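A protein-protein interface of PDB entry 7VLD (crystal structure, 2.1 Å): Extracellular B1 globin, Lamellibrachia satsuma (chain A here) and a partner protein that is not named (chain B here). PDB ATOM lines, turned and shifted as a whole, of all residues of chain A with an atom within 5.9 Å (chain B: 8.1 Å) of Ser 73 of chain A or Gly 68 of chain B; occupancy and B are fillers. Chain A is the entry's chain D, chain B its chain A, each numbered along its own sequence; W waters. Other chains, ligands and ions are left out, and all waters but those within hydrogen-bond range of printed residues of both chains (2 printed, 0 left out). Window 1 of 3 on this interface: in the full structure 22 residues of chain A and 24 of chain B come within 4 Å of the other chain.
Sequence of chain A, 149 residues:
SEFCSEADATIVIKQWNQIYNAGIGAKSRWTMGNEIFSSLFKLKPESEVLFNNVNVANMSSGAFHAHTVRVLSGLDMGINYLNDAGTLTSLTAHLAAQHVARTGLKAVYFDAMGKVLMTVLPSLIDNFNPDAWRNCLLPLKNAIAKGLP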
ATOM      1  N   TYR A  20      22.909 -19.055   9.752  1.00  0.00           N
ATOM      2  CA  TYR A  20      22.593 -17.838  10.493  1.00  0.00           C
ATOM      3  C   TYR A  20      21.183 -17.400  10.140  1.00  0.00           C
ATOM      4  O   TYR A  20      20.884 -17.158   8.968  1.00  0.00           O
ATOM      5  CB  TYR A  20      23.596 -16.723  10.176  1.00  0.00           C
ATOM      6  CG  TYR A  20      23.430 -15.475  11.023  1.00  0.00           C
ATOM      7  CD1 TYR A  20      22.414 -14.561  10.764  1.00  0.00           C
ATOM      8  CD2 TYR A  20      24.297 -15.204  12.074  1.00  0.00           C
ATOM      9  CE1 TYR A  20      22.256 -13.428  11.534  1.00  0.00           C
ATOM     10  CE2 TYR A  20      24.149 -14.064  12.847  1.00  0.00           C
ATOM     11  CZ  TYR A  20      23.127 -13.180  12.569  1.00  0.00           C
ATOM     12  OH  TYR A  20      22.965 -12.042  13.328  1.00  0.00           O
ATOM     13  N   THR A  68      30.932  -9.652  18.563  1.00  0.00           N
ATOM     14  CA  THR A  68      30.855 -10.550  17.414  1.00  0.00           C
ATOM     15  C   THR A  68      29.415 -10.728  16.953  1.00  0.00           C
ATOM     16  O   THR A  68      29.154 -10.850  15.750  1.00  0.00           O
ATOM     17  CB  THR A  68      31.486 -11.902  17.751  1.00  0.00           C
ATOM     18  OG1 THR A  68      30.694 -12.577  18.736  1.00  0.00           O
ATOM     19  CG2 THR A  68      32.900 -11.709  18.283  1.00  0.00           C
ATOM     20  N   VAL A  69      28.468 -10.744  17.893  1.00  0.00           N
ATOM     21  CA  VAL A  69      27.054 -10.756  17.525  1.00  0.00           C
ATOM     22  C   VAL A  69      26.706  -9.510  16.721  1.00  0.00           C
ATOM     23  O   VAL A  69      25.963  -9.577  15.734  1.00  0.00           O
ATOM     24  CB  VAL A  69      26.177 -10.890  18.784  1.00  0.00           C
ATOM     25  CG1 VAL A  69      24.717 -10.623  18.451  1.00  0.00           C
ATOM     26  CG2 VAL A  69      26.338 -12.272  19.397  1.00  0.00           C
ATOM     27  N   ARG A  70      27.247  -8.355  17.122  1.00  0.00           N
ATOM     28  CA  ARG A  70      27.023  -7.134  16.354  1.00  0.00           C
ATOM     29  C   ARG A  70      27.656  -7.223  14.972  1.00  0.00           C
ATOM     30  O   ARG A  70      27.069  -6.768  13.983  1.00  0.00           O
ATOM     31  CB  ARG A  70      27.567  -5.921  17.110  1.00  0.00           C
ATOM     32  CG  ARG A  70      26.652  -5.406  18.207  1.00  0.00           C
ATOM     33  CD  ARG A  70      27.029  -3.997  18.645  1.00  0.00           C
ATOM     34  NE  ARG A  70      28.325  -3.952  19.314  1.00  0.00           N
ATOM     35  CZ  ARG A  70      28.508  -4.199  20.607  1.00  0.00           C
ATOM     36  NH1 ARG A  70      29.725  -4.134  21.129  1.00  0.00           N
ATOM     37  NH2 ARG A  70      27.477  -4.516  21.380  1.00  0.00           N
ATOM     38  N   VAL A  71      28.853  -7.804  14.883  1.00  0.00           N
ATOM     39  CA  VAL A  71      29.550  -7.880  13.602  1.00  0.00           C
ATOM     40  C   VAL A  71      28.817  -8.816  12.651  1.00  0.00           C
ATOM     41  O   VAL A  71      28.578  -8.480  11.484  1.00  0.00           O
ATOM     42  CB  VAL A  71      31.009  -8.322  13.813  1.00  0.00           C
ATOM     43  CG1 VAL A  71      31.678  -8.597  12.475  1.00  0.00           C
ATOM     44  CG2 VAL A  71      31.773  -7.261  14.591  1.00  0.00           C
ATOM     45  N   LEU A  72      28.446 -10.005  13.133  1.00  0.00           N
ATOM     46  CA  LEU A  72      27.760 -10.963  12.272  1.00  0.00           C
ATOM     47  C   LEU A  72      26.364 -10.481  11.892  1.00  0.00           C
ATOM     48  O   LEU A  72      25.870 -10.818  10.810  1.00  0.00           O
ATOM     49  CB  LEU A  72      27.698 -12.327  12.957  1.00  0.00           C
ATOM     50  CG  LEU A  72      29.058 -12.981  13.213  1.00  0.00           C
ATOM     51  CD1 LEU A  72      28.894 -14.284  13.970  1.00  0.00           C
ATOM     52  CD2 LEU A  72      29.813 -13.207  11.909  1.00  0.00           C
ATOM     53  N   SER A  73      25.719  -9.689  12.754  1.00  0.00           N
ATOM     54  CA  SER A  73      24.431  -9.106  12.389  1.00  0.00           C
ATOM     55  C   SER A  73      24.589  -8.095  11.260  1.00  0.00           C
ATOM     56  O   SER A  73      23.743  -8.022  10.362  1.00  0.00           O
ATOM     57  CB  SER A  73      23.780  -8.452  13.610  1.00  0.00           C
ATOM     58  OG  SER A  73      22.495  -7.940  13.293  1.00  0.00           O
ATOM     59  N   GLY A  74      25.665  -7.306  11.289  1.00  0.00           N
ATOM     60  CA  GLY A  74      25.931  -6.400  10.183  1.00  0.00           C
ATOM     61  C   GLY A  74      26.236  -7.139   8.893  1.00  0.00           C
ATOM     62  O   GLY A  74      25.780  -6.741   7.817  1.00  0.00           O
ATOM     63  N   LEU A  75      27.009  -8.223   8.983  1.00  0.00           N
ATOM     64  CA  LEU A  75      27.260  -9.049   7.808  1.00  0.00           C
ATOM     65  C   LEU A  75      25.971  -9.682   7.303  1.00  0.00           C
ATOM     66  O   LEU A  75      25.736  -9.752   6.091  1.00  0.00           O
ATOM     67  CB  LEU A  75      28.299 -10.124   8.136  1.00  0.00           C
ATOM     68  CG  LEU A  75      28.609 -11.145   7.040  1.00  0.00           C
ATOM     69  CD1 LEU A  75      29.155 -10.452   5.800  1.00  0.00           C
ATOM     70  CD2 LEU A  75      29.581 -12.202   7.543  1.00  0.00           C
ATOM     71  N   ASP A  76      25.118 -10.142   8.222  1.00  0.00           N
ATOM     72  CA  ASP A  76      23.823 -10.687   7.831  1.00  0.00           C
ATOM     73  C   ASP A  76      22.960  -9.629   7.161  1.00  0.00           C
ATOM     74  O   ASP A  76      22.223  -9.922   6.211  1.00  0.00           O
ATOM     75  CB  ASP A  76      23.107 -11.253   9.054  1.00  0.00           C
ATOM     76  CG  ASP A  76      21.691 -11.691   8.747  1.00  0.00           C
ATOM     77  OD1 ASP A  76      21.517 -12.807   8.219  1.00  0.00           O
ATOM     78  OD2 ASP A  76      20.753 -10.915   9.030  1.00  0.00           O
ATOM     79  N   MET A  77      23.031  -8.393   7.654  1.00  0.00           N
ATOM     80  CA  MET A  77      22.248  -7.308   7.078  1.00  0.00           C
ATOM     81  C   MET A  77      22.691  -7.003   5.653  1.00  0.00           C
ATOM     82  O   MET A  77      21.853  -6.812   4.764  1.00  0.00           O
ATOM     83  CB  MET A  77      22.371  -6.074   7.966  1.00  0.00           C
ATOM     84  CG  MET A  77      21.577  -4.871   7.522  1.00  0.00           C
ATOM     85  SD  MET A  77      21.759  -3.560   8.744  1.00  0.00           S
ATOM     86  CE  MET A  77      23.537  -3.351   8.744  1.00  0.00           C
ATOM     87  N   GLY A  78      24.003  -6.955   5.417  1.00  0.00           N
ATOM     88  CA  GLY A  78      24.490  -6.716   4.068  1.00  0.00           C
ATOM     89  C   GLY A  78      24.116  -7.828   3.107  1.00  0.00           C
ATOM     90  O   GLY A  78      23.723  -7.570   1.967  1.00  0.00           O
ATOM     91  N   TRP B  14       9.303 -14.369  17.113  1.00  0.00           N
ATOM     92  CA  TRP B  14      10.058 -13.382  16.347  1.00  0.00           C
ATOM     93  C   TRP B  14      10.626 -13.995  15.074  1.00  0.00           C
ATOM     94  O   TRP B  14      10.470 -13.438  13.982  1.00  0.00           O
ATOM     95  CB  TRP B  14      11.177 -12.788  17.201  1.00  0.00           C
ATOM     96  CG  TRP B  14      12.210 -12.067  16.391  1.00  0.00           C
ATOM     97  CD1 TRP B  14      13.454 -12.521  16.058  1.00  0.00           C
ATOM     98  CD2 TRP B  14      12.084 -10.771  15.797  1.00  0.00           C
ATOM     99  NE1 TRP B  14      14.112 -11.584  15.301  1.00  0.00           N
ATOM    100  CE2 TRP B  14      13.293 -10.499  15.125  1.00  0.00           C
ATOM    101  CE3 TRP B  14      11.069  -9.810  15.769  1.00  0.00           C
ATOM    102  CZ2 TRP B  14      13.514  -9.309  14.437  1.00  0.00           C
ATOM    103  CZ3 TRP B  14      11.289  -8.630  15.084  1.00  0.00           C
ATOM    104  CH2 TRP B  14      12.502  -8.390  14.426  1.00  0.00           C
ATOM    105  N   TYR B  18       9.668 -12.606  11.503  1.00  0.00           N
ATOM    106  CA  TYR B  18      10.763 -11.855  10.896  1.00  0.00           C
ATOM    107  C   TYR B  18      11.092 -12.367   9.498  1.00  0.00           C
ATOM    108  O   TYR B  18      11.283 -11.570   8.573  1.00  0.00           O
ATOM    109  CB  TYR B  18      11.986 -11.931  11.811  1.00  0.00           C
ATOM    110  CG  TYR B  18      13.155 -11.044  11.459  1.00  0.00           C
ATOM    111  CD1 TYR B  18      12.979  -9.703  11.145  1.00  0.00           C
ATOM    112  CD2 TYR B  18      14.449 -11.546  11.492  1.00  0.00           C
ATOM    113  CE1 TYR B  18      14.063  -8.894  10.846  1.00  0.00           C
ATOM    114  CE2 TYR B  18      15.533 -10.749  11.195  1.00  0.00           C
ATOM    115  CZ  TYR B  18      15.336  -9.425  10.874  1.00  0.00           C
ATOM    116  OH  TYR B  18      16.423  -8.633  10.582  1.00  0.00           O
ATOM    117  N   ARG B  24      12.025  -9.562   5.223  1.00  0.00           N
ATOM    118  CA  ARG B  24      12.609  -8.812   6.327  1.00  0.00           C
ATOM    119  C   ARG B  24      12.398  -7.313   6.148  1.00  0.00           C
ATOM    120  O   ARG B  24      12.029  -6.612   7.098  1.00  0.00           O
ATOM    121  CB  ARG B  24      14.094  -9.156   6.422  1.00  0.00           C
ATOM    122  CG  ARG B  24      14.889  -8.423   7.463  1.00  0.00           C
ATOM    123  CD  ARG B  24      16.244  -9.091   7.580  1.00  0.00           C
ATOM    124  NE  ARG B  24      16.090 -10.528   7.798  1.00  0.00           N
ATOM    125  CZ  ARG B  24      17.098 -11.366   8.021  1.00  0.00           C
ATOM    126  NH1 ARG B  24      18.342 -10.915   8.062  1.00  0.00           N
ATOM    127  NH2 ARG B  24      16.857 -12.657   8.207  1.00  0.00           N
ATOM    128  N   ALA B  61      17.874   1.828   4.999  1.00  0.00           N
ATOM    129  CA  ALA B  61      19.069   1.421   5.732  1.00  0.00           C
ATOM    130  C   ALA B  61      18.860   1.549   7.234  1.00  0.00           C
ATOM    131  O   ALA B  61      19.283   0.676   8.002  1.00  0.00           O
ATOM    132  CB  ALA B  61      20.271   2.251   5.284  1.00  0.00           C
ATOM    133  N   HIS B  62      18.213   2.632   7.671  1.00  0.00           N
ATOM    134  CA  HIS B  62      17.901   2.787   9.087  1.00  0.00           C
ATOM    135  C   HIS B  62      16.968   1.682   9.565  1.00  0.00           C
ATOM    136  O   HIS B  62      17.175   1.107  10.641  1.00  0.00           O
ATOM    137  CB  HIS B  62      17.279   4.160   9.339  1.00  0.00           C
ATOM    138  CG  HIS B  62      16.778   4.347  10.736  1.00  0.00           C
ATOM    139  ND1 HIS B  62      17.623   4.518  11.812  1.00  0.00           N
ATOM    140  CD2 HIS B  62      15.521   4.382  11.234  1.00  0.00           C
ATOM    141  CE1 HIS B  62      16.906   4.656  12.913  1.00  0.00           C
ATOM    142  NE2 HIS B  62      15.628   4.578  12.590  1.00  0.00           N
ATOM    143  N   ILE B  63      15.936   1.373   8.776  1.00  0.00           N
ATOM    144  CA  ILE B  63      15.030   0.277   9.113  1.00  0.00           C
ATOM    145  C   ILE B  63      15.811  -1.021   9.284  1.00  0.00           C
ATOM    146  O   ILE B  63      15.612  -1.764  10.252  1.00  0.00           O
ATOM    147  CB  ILE B  63      13.938   0.132   8.039  1.00  0.00           C
ATOM    148  CG1 ILE B  63      12.992   1.335   8.061  1.00  0.00           C
ATOM    149  CG2 ILE B  63      13.174  -1.164   8.231  1.00  0.00           C
ATOM    150  CD1 ILE B  63      11.883   1.249   7.034  1.00  0.00           C
ATOM    151  N   ALA B  64      16.715  -1.306   8.344  1.00  0.00           N
ATOM    152  CA  ALA B  64      17.491  -2.541   8.406  1.00  0.00           C
ATOM    153  C   ALA B  64      18.327  -2.608   9.679  1.00  0.00           C
ATOM    154  O   ALA B  64      18.399  -3.660  10.325  1.00  0.00           O
ATOM    155  CB  ALA B  64      18.384  -2.661   7.172  1.00  0.00           C
ATOM    156  N   ARG B  65      18.960  -1.496  10.057  1.00  0.00           N
ATOM    157  CA  ARG B  65      19.781  -1.491  11.264  1.00  0.00           C
ATOM    158  C   ARG B  65      18.935  -1.717  12.511  1.00  0.00           C
ATOM    159  O   ARG B  65      19.342  -2.456  13.415  1.00  0.00           O
ATOM    160  CB  ARG B  65      20.557  -0.177  11.373  1.00  0.00           C
ATOM    161  CG  ARG B  65      21.754  -0.080  10.437  1.00  0.00           C
ATOM    162  CD  ARG B  65      22.638   1.115  10.774  1.00  0.00           C
ATOM    163  NE  ARG B  65      21.985   2.389  10.484  1.00  0.00           N
ATOM    164  CZ  ARG B  65      22.010   2.986   9.296  1.00  0.00           C
ATOM    165  NH1 ARG B  65      22.652   2.421   8.282  1.00  0.00           N
ATOM    166  NH2 ARG B  65      21.391   4.144   9.120  1.00  0.00           N
ATOM    167  N   VAL B  66      17.755  -1.099  12.574  1.00  0.00           N
ATOM    168  CA  VAL B  66      16.927  -1.194  13.773  1.00  0.00           C
ATOM    169  C   VAL B  66      16.412  -2.616  13.959  1.00  0.00           C
ATOM    170  O   VAL B  66      16.553  -3.206  15.036  1.00  0.00           O
ATOM    171  CB  VAL B  66      15.774  -0.177  13.713  1.00  0.00           C
ATOM    172  CG1 VAL B  66      14.826  -0.384  14.882  1.00  0.00           C
ATOM    173  CG2 VAL B  66      16.321   1.242  13.717  1.00  0.00           C
ATOM    174  N   ILE B  67      15.805  -3.191  12.915  1.00  0.00           N
ATOM    175  CA  ILE B  67      15.287  -4.550  13.044  1.00  0.00           C
ATOM    176  C   ILE B  67      16.431  -5.548  13.183  1.00  0.00           C
ATOM    177  O   ILE B  67      16.290  -6.571  13.865  1.00  0.00           O
ATOM    178  CB  ILE B  67      14.359  -4.904  11.865  1.00  0.00           C
ATOM    179  CG1 ILE B  67      15.122  -4.908  10.538  1.00  0.00           C
ATOM    180  CG2 ILE B  67      13.180  -3.941  11.810  1.00  0.00           C
ATOM    181  CD1 ILE B  67      14.292  -5.377   9.361  1.00  0.00           C
ATOM    182  N   GLY B  68      17.576  -5.272  12.554  1.00  0.00           N
ATOM    183  CA  GLY B  68      18.760  -6.064  12.832  1.00  0.00           C
ATOM    184  C   GLY B  68      19.188  -5.968  14.281  1.00  0.00           C
ATOM    185  O   GLY B  68      19.682  -6.943  14.854  1.00  0.00           O
ATOM    186  N   GLY B  69      18.993  -4.800  14.897  1.00  0.00           N
ATOM    187  CA  GLY B  69      19.280  -4.666  16.316  1.00  0.00           C
ATOM    188  C   GLY B  69      18.308  -5.444  17.179  1.00  0.00           C
ATOM    189  O   GLY B  69      18.704  -6.062  18.171  1.00  0.00           O
ATOM    190  N   LEU B  70      17.021  -5.421  16.821  1.00  0.00           N
ATOM    191  CA  LEU B  70      16.047  -6.252  17.523  1.00  0.00           C
ATOM    192  C   LEU B  70      16.406  -7.726  17.414  1.00  0.00           C
ATOM    193  O   LEU B  70      16.326  -8.468  18.400  1.00  0.00           O
ATOM    194  CB  LEU B  70      14.644  -6.008  16.969  1.00  0.00           C
ATOM    195  CG  LEU B  70      13.864  -4.805  17.496  1.00  0.00           C
ATOM    196  CD1 LEU B  70      12.540  -4.677  16.758  1.00  0.00           C
ATOM    197  CD2 LEU B  70      13.636  -4.927  18.994  1.00  0.00           C
ATOM    198  N   ASP B  71      16.817  -8.167  16.222  1.00  0.00           N
ATOM    199  CA  ASP B  71      17.117  -9.579  16.010  1.00  0.00           C
ATOM    200  C   ASP B  71      18.271 -10.040  16.892  1.00  0.00           C
ATOM    201  O   ASP B  71      18.190 -11.091  17.540  1.00  0.00           O
ATOM    202  CB  ASP B  71      17.439  -9.827  14.537  1.00  0.00           C
ATOM    203  CG  ASP B  71      17.706 -11.287  14.245  1.00  0.00           C
ATOM    204  OD1 ASP B  71      16.749 -12.085  14.319  1.00  0.00           O
ATOM    205  OD2 ASP B  71      18.868 -11.638  13.950  1.00  0.00           O
ATOM    206  N   ARG B  72      19.359  -9.267  16.929  1.00  0.00           N
ATOM    207  CA  ARG B  72      20.524  -9.684  17.704  1.00  0.00           C
ATOM    208  C   ARG B  72      20.237  -9.641  19.201  1.00  0.00           C
ATOM    209  O   ARG B  72      20.703 -10.506  19.952  1.00  0.00           O
ATOM    210  CB  ARG B  72      21.732  -8.811  17.349  1.00  0.00           C
ATOM    211  CG  ARG B  72      21.664  -7.389  17.880  1.00  0.00           C
ATOM    212  CD  ARG B  72      22.776  -6.507  17.340  1.00  0.00           C
ATOM    213  NE  ARG B  72      23.128  -5.474  18.309  1.00  0.00           N
ATOM    214  CZ  ARG B  72      23.474  -4.229  17.995  1.00  0.00           C
ATOM    215  NH1 ARG B  72      23.508  -3.842  16.729  1.00  0.00           N
ATOM    216  NH2 ARG B  72      23.777  -3.368  18.956  1.00  0.00           N
ATOM    217  N   VAL B  73      19.456  -8.656  19.650  1.00  0.00           N
ATOM    218  CA  VAL B  73      19.118  -8.553  21.066  1.00  0.00           C
ATOM    219  C   VAL B  73      18.216  -9.708  21.483  1.00  0.00           C
ATOM    220  O   VAL B  73      18.427 -10.340  22.525  1.00  0.00           O
ATOM    221  CB  VAL B  73      18.462  -7.191  21.362  1.00  0.00           C
ATOM    222  CG1 VAL B  73      17.787  -7.209  22.724  1.00  0.00           C
ATOM    223  CG2 VAL B  73      19.495  -6.073  21.291  1.00  0.00           C
ATOM    224  N   ILE B  74      17.196  -9.999  20.672  1.00  0.00           N
ATOM    225  CA  ILE B  74      16.318 -11.131  20.953  1.00  0.00           C
ATOM    226  C   ILE B  74      17.111 -12.433  20.952  1.00  0.00           C
ATOM    227  O   ILE B  74      16.878 -13.321  21.782  1.00  0.00           O
ATOM    228  CB  ILE B  74      15.155 -11.166  19.942  1.00  0.00           C
ATOM    229  CG1 ILE B  74      14.210  -9.983  20.178  1.00  0.00           C
ATOM    230  CG2 ILE B  74      14.401 -12.488  20.022  1.00  0.00           C
ATOM    231  CD1 ILE B  74      13.079  -9.884  19.176  1.00  0.00           C
ATOM    232  N   SER B  75      18.075 -12.559  20.036  1.00  0.00           N
ATOM    233  CA  SER B  75      18.867 -13.782  19.963  1.00  0.00           C
ATOM    234  C   SER B  75      19.704 -13.988  21.217  1.00  0.00           C
ATOM    235  O   SER B  75      19.985 -15.131  21.595  1.00  0.00           O
ATOM    236  CB  SER B  75      19.767 -13.760  18.725  1.00  0.00           C
ATOM    237  OG  SER B  75      20.938 -12.996  18.957  1.00  0.00           O
ATOM    238  N   MET B  76      20.110 -12.903  21.875  1.00  0.00           N
ATOM    239  CA  MET B  76      20.898 -12.975  23.098  1.00  0.00           C
ATOM    240  C   MET B  76      20.038 -13.002  24.357  1.00  0.00           C
ATOM    241  O   MET B  76      20.565 -12.793  25.455  1.00  0.00           O
ATOM    242  CB  MET B  76      21.878 -11.799  23.165  1.00  0.00           C
ATOM    243  CG  MET B  76      23.025 -11.886  22.169  1.00  0.00           C
ATOM    244  SD  MET B  76      24.146 -10.473  22.251  1.00  0.00           S
ATOM    245  CE  MET B  76      23.113  -9.182  21.565  1.00  0.00           C
ATOM    246  N   ASP B  86      25.282  -5.577  25.161  1.00  0.00           N
ATOM    247  CA  ASP B  86      24.783  -4.964  23.934  1.00  0.00           C
ATOM    248  C   ASP B  86      23.729  -3.906  24.235  1.00  0.00           C
ATOM    249  O   ASP B  86      23.663  -2.879  23.550  1.00  0.00           O
ATOM    250  CB  ASP B  86      24.230  -6.039  22.998  1.00  0.00           C
ATOM    251  CG  ASP B  86      24.044  -5.536  21.579  1.00  0.00           C
ATOM    252  OD1 ASP B  86      24.931  -4.809  21.083  1.00  0.00           O
ATOM    253  OD2 ASP B  86      23.019  -5.880  20.953  1.00  0.00           O
ATOM    254  N   LEU B  90      23.704  -0.068  23.050  1.00  0.00           N
ATOM    255  CA  LEU B  90      22.616   0.673  22.422  1.00  0.00           C
ATOM    256  C   LEU B  90      22.256   1.914  23.230  1.00  0.00           C
ATOM    257  O   LEU B  90      21.933   2.962  22.658  1.00  0.00           O
ATOM    258  CB  LEU B  90      21.397  -0.234  22.249  1.00  0.00           C
ATOM    259  CG  LEU B  90      21.586  -1.394  21.268  1.00  0.00           C
ATOM    260  CD1 LEU B  90      20.482  -2.430  21.423  1.00  0.00           C
ATOM    261  CD2 LEU B  90      21.638  -0.873  19.841  1.00  0.00           C
HETATM  262  O   HOH W   1      20.880 -10.031  12.998  1.00  0.00           O
HETATM  263  O   HOH W   2      22.642  -5.310  14.162  1.00  0.00           O
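The guanidinium group of Arg 24 of chain B is in salt-bridge range of the side-chain carboxylate of Asp 76 of chain A, at 2.6 Å. The backbone NH of Arg 65 of chain B sits at hydrogen-bond distance from the side-chain sulfur of Met 77 of chain A (3.7 Å). The side-chain hydroxyl (OG) of Ser 73 of chain A sits at hydrogen-bond distance from the backbone carbonyl oxygen (O) of Gly 68 of chain B, 3.4 Å away. The side-chain carboxylate of Asp 86 of chain B is in salt-bridge range of the guanidinium group of Arg 70 of chain A (2.6 Å). The side-chain sulfur (SD) of Met 77 of chain A lies close to the backbone carbonyl oxygen (O) of Ala 64 of chain B (3.7 Å).
OH of Tyr 18 of chain B sits close to NE of Arg 24 of chain B. The backbone carbonyl oxygen (O) of Arg 72 of chain B is in hydrogen-bond range of the side-chain hydroxyl (OG) of Ser 75 of chain B (2.7 Å). NE of Arg 72 of chain B is in salt-bridge range of OD2 of Asp 86 of chain B (2.7 Å).
Water W1 lies within hydrogen-bond range of the side-chain hydroxyl (OG) of Ser 73 of chain A (2.7 Å), the side-chain carboxylate (OD2) of Asp 71 of chain B (2.7 Å) and the side-chain hydroxyl (OH) of Tyr 20 of chain A (2.9 Å). Water W2 lies within hydrogen-bond range of OG of Ser 73 of chain A (2.8 Å), NH1 of Arg 72 of chain B (3.1 Å) and O of Gly 68 of chain B (3.5 Å).
Among the printed residues, pairs that only touch across the chains: Val 69 of chain A with Arg 72 of chain B, Val 69 of chain A with Met 76 of chain B and Arg 70 of chain A with Arg 72 of chain B.
Of the 12 printed residues of chain A, 5 touch a printed residue of chain B. Hydrophobic or aromatic side chains of chain A that line the printed part of chain B: Val 69 and Met 77. Of the 21 printed residues of chain B, 7 touch a printed residue of chain A. Hydrophobic or aromatic side chains of chain B that line the printed part of chain A: Ala 64 and Met 76.
Of chain B, only Gly 68 comes within 4 Å of Ser 73 of chain A. Of chain A, only Ser 73 comes within 4 Å of Gly 68 of chain B. Gly 74 of chain A touches none of the printed residues of chain B. Printed residues of chain A within 4 Å of Arg 24 of chain B: Asp 76 (2.6 Å). Of the printed residues of chain B, Arg 70 of chain A touches Arg 72 and Asp 86. Of the printed residues of chain A, Arg 72 of chain B touches Val 69 and Arg 70. Of the printed residues of chain A, Met 76 of chain B touches Val 69. The nearest residue of chain B that does not touch Ser 73 of chain A is Arg 72 of chain B (4.2 Å). The nearest residue of chain A that does not touch Gly 68 of chain B is Met 77 of chain A (5.7 Å).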
